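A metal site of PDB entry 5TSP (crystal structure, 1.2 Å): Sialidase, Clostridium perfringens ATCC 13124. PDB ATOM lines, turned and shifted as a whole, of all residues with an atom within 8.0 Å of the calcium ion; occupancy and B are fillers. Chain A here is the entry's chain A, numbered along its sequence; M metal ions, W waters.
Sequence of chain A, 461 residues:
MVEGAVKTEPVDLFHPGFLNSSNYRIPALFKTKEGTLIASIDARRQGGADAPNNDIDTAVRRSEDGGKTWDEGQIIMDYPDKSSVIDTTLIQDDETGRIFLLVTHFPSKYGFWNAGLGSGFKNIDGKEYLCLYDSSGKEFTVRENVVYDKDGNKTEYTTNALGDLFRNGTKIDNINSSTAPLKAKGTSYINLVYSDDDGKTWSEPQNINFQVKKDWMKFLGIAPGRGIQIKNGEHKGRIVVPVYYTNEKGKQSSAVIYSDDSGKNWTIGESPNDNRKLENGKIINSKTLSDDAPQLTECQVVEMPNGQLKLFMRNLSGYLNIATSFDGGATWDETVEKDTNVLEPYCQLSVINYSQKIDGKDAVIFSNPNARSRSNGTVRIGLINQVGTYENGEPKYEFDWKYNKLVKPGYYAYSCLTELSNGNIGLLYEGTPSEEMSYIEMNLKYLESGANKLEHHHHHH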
ATOM      1  N   ALA A  43      22.554  10.253  20.477  1.00  0.00           N
ATOM      2  CA  ALA A  43      22.237   8.909  20.942  1.00  0.00           C
ATOM      3  C   ALA A  43      23.228   7.981  20.241  1.00  0.00           C
ATOM      4  O   ALA A  43      23.077   7.637  19.070  1.00  0.00           O
ATOM      5  CB  ALA A  43      20.802   8.545  20.596  1.00  0.00           C
ATOM      6  N   ARG A  45      24.678   4.694  19.584  1.00  0.00           N
ATOM      7  CA  ARG A  45      24.008   3.396  19.673  1.00  0.00           C
ATOM      8  C   ARG A  45      24.936   2.205  19.860  1.00  0.00           C
ATOM      9  O   ARG A  45      24.500   1.145  20.313  1.00  0.00           O
ATOM     10  CB  ARG A  45      23.176   3.152  18.405  1.00  0.00           C
ATOM     11  CG  ARG A  45      22.137   4.199  18.098  1.00  0.00           C
ATOM     12  CD  ARG A  45      21.004   4.091  19.068  1.00  0.00           C
ATOM     13  NE  ARG A  45      19.788   4.772  18.634  1.00  0.00           N
ATOM     14  CZ  ARG A  45      18.621   4.642  19.245  1.00  0.00           C
ATOM     15  NH1 ARG A  45      18.532   3.835  20.301  1.00  0.00           N
ATOM     16  NH2 ARG A  45      17.551   5.294  18.816  1.00  0.00           N
ATOM     17  N   GLN A  46      26.183   2.349  19.484  1.00  0.00           N
ATOM     18  CA  GLN A  46      27.131   1.244  19.518  1.00  0.00           C
ATOM     19  C   GLN A  46      28.330   1.602  20.287  1.00  0.00           C
ATOM     20  O   GLN A  46      29.398   1.561  19.764  1.00  0.00           O
ATOM     21  CB  GLN A  46      27.476   0.887  18.016  1.00  0.00           C
ATOM     22  CG  GLN A  46      26.269   0.374  17.253  1.00  0.00           C
ATOM     23  CD  GLN A  46      26.489   0.035  15.799  1.00  0.00           C
ATOM     24  OE1 GLN A  46      27.510   0.145  15.345  1.00  0.00           O
ATOM     25  NE2 GLN A  46      25.465  -0.278  15.132  1.00  0.00           N
ATOM     26  N   ASN A  54      30.865   4.036  15.127  1.00  0.00           N
ATOM     27  CA  ASN A  54      29.587   4.073  15.814  1.00  0.00           C
ATOM     28  C   ASN A  54      28.452   4.153  14.805  1.00  0.00           C
ATOM     29  O   ASN A  54      28.695   4.196  13.600  1.00  0.00           O
ATOM     30  CB  ASN A  54      29.541   5.267  16.774  1.00  0.00           C
ATOM     31  CG  ASN A  54      28.798   4.966  18.048  1.00  0.00           C
ATOM     32  OD1 ASN A  54      27.760   4.280  18.028  1.00  0.00           O
ATOM     33  ND2 ASN A  54      29.310   5.469  19.170  1.00  0.00           N
ATOM     34  N   ASP A  55      27.244   4.170  15.326  1.00  0.00           N
ATOM     35  CA  ASP A  55      26.043   4.499  14.573  1.00  0.00           C
ATOM     36  C   ASP A  55      25.283   5.442  15.495  1.00  0.00           C
ATOM     37  O   ASP A  55      24.752   5.018  16.529  1.00  0.00           O
ATOM     38  CB  ASP A  55      25.249   3.228  14.258  1.00  0.00           C
ATOM     39  CG  ASP A  55      24.116   3.460  13.283  1.00  0.00           C
ATOM     40  OD1 ASP A  55      23.881   2.604  12.397  1.00  0.00           O
ATOM     41  OD2 ASP A  55      23.451   4.509  13.425  1.00  0.00           O
ATOM     42  N   ILE A  56      25.269   6.724  15.166  1.00  0.00           N
ATOM     43  CA  ILE A  56      24.778   7.762  16.078  1.00  0.00           C
ATOM     44  C   ILE A  56      23.567   8.472  15.485  1.00  0.00           C
ATOM     45  O   ILE A  56      23.567   8.857  14.315  1.00  0.00           O
ATOM     46  CB  ILE A  56      25.883   8.804  16.385  1.00  0.00           C
ATOM     47  CG1 ILE A  56      27.173   8.109  16.848  1.00  0.00           C
ATOM     48  CG2 ILE A  56      25.386   9.833  17.391  1.00  0.00           C
ATOM     49  CD1 ILE A  56      28.390   9.024  16.909  1.00  0.00           C
ATOM     50  N   ASP A  57      22.532   8.604  16.312  1.00  0.00           N
ATOM     51  CA  ASP A  57      21.284   9.275  15.951  1.00  0.00           C
ATOM     52  C   ASP A  57      21.147  10.538  16.801  1.00  0.00           C
ATOM     53  O   ASP A  57      21.810  10.656  17.829  1.00  0.00           O
ATOM     54  CB  ASP A  57      20.086   8.367  16.243  1.00  0.00           C
ATOM     55  CG  ASP A  57      20.168   7.030  15.533  1.00  0.00           C
ATOM     56  OD1 ASP A  57      19.590   6.051  16.070  1.00  0.00           O
ATOM     57  OD2 ASP A  57      20.796   6.933  14.458  1.00  0.00           O
ATOM     58  N   THR A  58      20.292  11.473  16.394  1.00  0.00           N
ATOM     59  CA  THR A  58      20.046  12.678  17.189  1.00  0.00           C
ATOM     60  C   THR A  58      18.759  12.548  17.989  1.00  0.00           C
ATOM     61  O   THR A  58      17.699  12.256  17.404  1.00  0.00           O
ATOM     62  CB  THR A  58      19.905  13.914  16.293  1.00  0.00           C
ATOM     63  OG1 THR A  58      21.105  14.105  15.533  1.00  0.00           O
ATOM     64  CG2 THR A  58      19.622  15.156  17.127  1.00  0.00           C
ATOM     65  N   ILE A  75      13.680  10.609  18.518  1.00  0.00           N
ATOM     66  CA  ILE A  75      14.815  10.575  17.601  1.00  0.00           C
ATOM     67  C   ILE A  75      14.415  11.357  16.373  1.00  0.00           C
ATOM     68  O   ILE A  75      13.360  11.075  15.780  1.00  0.00           O
ATOM     69  CB  ILE A  75      15.151   9.135  17.185  1.00  0.00           C
ATOM     70  CG1 ILE A  75      15.538   8.305  18.408  1.00  0.00           C
ATOM     71  CG2 ILE A  75      16.245   9.108  16.123  1.00  0.00           C
ATOM     72  CD1 ILE A  75      16.797   8.772  19.083  1.00  0.00           C
ATOM     73  N   MET A  77      16.873  12.392  13.753  1.00  0.00           N
ATOM     74  CA  MET A  77      17.692  12.022  12.601  1.00  0.00           C
ATOM     75  C   MET A  77      18.340  10.677  12.890  1.00  0.00           C
ATOM     76  O   MET A  77      18.813  10.450  14.012  1.00  0.00           O
ATOM     77  CB  MET A  77      18.748  13.077  12.276  1.00  0.00           C
ATOM     78  CG  MET A  77      18.222  14.262  11.464  1.00  0.00           C
ATOM     79  SD  MET A  77      19.443  15.564  11.228  1.00  0.00           S
ATOM     80  CE  MET A  77      19.371  16.333  12.852  1.00  0.00           C
ATOM     81  N   ASP A  78      18.359   9.808  11.890  1.00  0.00           N
ATOM     82  CA  ASP A  78      18.843   8.440  12.038  1.00  0.00           C
ATOM     83  C   ASP A  78      19.155   7.933  10.641  1.00  0.00           C
ATOM     84  O   ASP A  78      18.255   7.804   9.809  1.00  0.00           O
ATOM     85  CB  ASP A  78      17.749   7.607  12.695  1.00  0.00           C
ATOM     86  CG  ASP A  78      18.025   6.104  12.695  1.00  0.00           C
ATOM     87  OD1 ASP A  78      17.138   5.363  13.154  1.00  0.00           O
ATOM     88  OD2 ASP A  78      19.103   5.647  12.236  1.00  0.00           O
ATOM     89  N   TYR A  79      20.424   7.673  10.368  1.00  0.00           N
ATOM     90  CA  TYR A  79      20.863   7.096   9.106  1.00  0.00           C
ATOM     91  C   TYR A  79      21.285   5.651   9.348  1.00  0.00           C
ATOM     92  O   TYR A  79      21.633   5.271  10.462  1.00  0.00           O
ATOM     93  CB  TYR A  79      22.021   7.913   8.529  1.00  0.00           C
ATOM     94  CG  TYR A  79      21.600   9.288   8.083  1.00  0.00           C
ATOM     95  CD1 TYR A  79      21.180   9.521   6.778  1.00  0.00           C
ATOM     96  CD2 TYR A  79      21.622  10.357   8.972  1.00  0.00           C
ATOM     97  CE1 TYR A  79      20.796  10.767   6.366  1.00  0.00           C
ATOM     98  CE2 TYR A  79      21.236  11.613   8.571  1.00  0.00           C
ATOM     99  CZ  TYR A  79      20.826  11.812   7.269  1.00  0.00           C
ATOM    100  OH  TYR A  79      20.459  13.081   6.887  1.00  0.00           O
ATOM    101  N   PRO A  80      21.214   4.810   8.312  1.00  0.00           N
ATOM    102  CA  PRO A  80      21.485   3.391   8.504  1.00  0.00           C
ATOM    103  C   PRO A  80      22.964   3.035   8.475  1.00  0.00           C
ATOM    104  O   PRO A  80      23.807   3.810   8.009  1.00  0.00           O
ATOM    105  CB  PRO A  80      20.784   2.751   7.296  1.00  0.00           C
ATOM    106  CG  PRO A  80      20.908   3.768   6.234  1.00  0.00           C
ATOM    107  CD  PRO A  80      20.764   5.102   6.931  1.00  0.00           C
ATOM    108  N   ASP A  81      23.270   1.841   8.985  1.00  0.00           N
ATOM    109  CA  ASP A  81      24.531   1.150   8.673  1.00  0.00           C
ATOM    110  C   ASP A  81      25.778   1.963   9.002  1.00  0.00           C
ATOM    111  O   ASP A  81      26.703   2.054   8.208  1.00  0.00           O
ATOM    112  CB  ASP A  81      24.525   0.717   7.203  1.00  0.00           C
ATOM    113  CG  ASP A  81      25.649  -0.257   6.867  1.00  0.00           C
ATOM    114  OD1 ASP A  81      26.073  -1.028   7.760  1.00  0.00           O
ATOM    115  OD2 ASP A  81      26.102  -0.245   5.702  1.00  0.00           O
ATOM    116  N   LYS A  82      25.789   2.540  10.206  1.00  0.00           N
ATOM    117  CA  LYS A  82      26.942   3.258  10.756  1.00  0.00           C
ATOM    118  C   LYS A  82      27.259   4.560  10.031  1.00  0.00           C
ATOM    119  O   LYS A  82      28.359   5.103  10.150  1.00  0.00           O
ATOM    120  CB  LYS A  82      28.177   2.348  10.872  1.00  0.00           C
ATOM    121  CG  LYS A  82      27.931   1.107  11.722  1.00  0.00           C
ATOM    122  CD  LYS A  82      29.195   0.258  11.872  1.00  0.00           C
ATOM    123  CE  LYS A  82      30.233   0.939  12.742  1.00  0.00           C
ATOM    124  NZ  LYS A  82      31.525   0.172  12.742  1.00  0.00           N
ATOM    125  N   SER A  83      26.276   5.106   9.323  1.00  0.00           N
ATOM    126  CA  SER A  83      26.281   6.528   9.003  1.00  0.00           C
ATOM    127  C   SER A  83      25.781   7.248  10.252  1.00  0.00           C
ATOM    128  O   SER A  83      24.805   6.815  10.873  1.00  0.00           O
ATOM    129  CB  SER A  83      25.355   6.801   7.820  1.00  0.00           C
ATOM    130  OG  SER A  83      25.247   8.194   7.563  1.00  0.00           O
ATOM    131  N   SER A  84      26.437   8.340  10.630  1.00  0.00           N
ATOM    132  CA  SER A  84      26.144   9.037  11.875  1.00  0.00           C
ATOM    133  C   SER A  84      25.837  10.505  11.701  1.00  0.00           C
ATOM    134  O   SER A  84      26.409  11.179  10.847  1.00  0.00           O
ATOM    135  CB  SER A  84      27.340   8.946  12.833  1.00  0.00           C
ATOM    136  OG  SER A  84      27.458   7.643  13.364  1.00  0.00           O
ATOM    137  N   VAL A  85      24.955  10.998  12.570  1.00  0.00           N
ATOM    138  CA  VAL A  85      24.812  12.425  12.827  1.00  0.00           C
ATOM    139  C   VAL A  85      25.424  12.695  14.191  1.00  0.00           C
ATOM    140  O   VAL A  85      25.134  11.975  15.146  1.00  0.00           O
ATOM    141  CB  VAL A  85      23.338  12.915  12.752  1.00  0.00           C
ATOM    142  CG1 VAL A  85      22.964  13.185  11.303  1.00  0.00           C
ATOM    143  CG2 VAL A  85      22.372  11.907  13.371  1.00  0.00           C
HETATM  144 CA    CA M   1      21.313   5.252  12.820  1.00  0.00          CA
HETATM  145  O   HOH W   1      21.178   2.879  12.112  1.00  0.00           O
HETATM  146  O   HOH W   2      20.382   3.986  14.678  1.00  0.00           O
HETATM  147  O   HOH W   3      22.519   7.333  12.283  1.00  0.00           O
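The calcium ion is bound by OD2 of Asp 78 (2.3 Å), OD2 of Asp 55 (2.3 Å), O of Tyr 79 (2.4 Å), OD2 of Asp 57 (2.4 Å), water W2 (2.4 Å), water W3 (2.5 Å) and water W1 (2.5 Å). The calcium ion has seven donor atoms within binding distance.
Water W3 lies within hydrogen-bond range of the backbone carbonyl oxygen of Ser 83 (2.7 Å), the backbone carbonyl oxygen of Ile 56 (2.7 Å) and the backbone NH of Tyr 79 (2.9 Å).
The backbone NH (N) of Arg 45 sits at hydrogen-bond distance from the backbone carbonyl oxygen (O) of Asp 55. OD1 of Asp 55 is in hydrogen-bond range of N of Lys 82. The side-chain carboxylate of Asp 57 lies within salt-bridge range of the guanidinium group of Arg 45 (2.9 Å). The backbone carbonyl oxygen of Asp 57 is in hydrogen-bond range of the backbone NH of Ala 43 (2.8 Å).
Four residues have an atom within 4 Å of the calcium ion: Asp 55, Asp 57, Asp 78 and Tyr 79. The nearest printed residue that does not touch the calcium ion is Ser 83 (4.3 Å).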
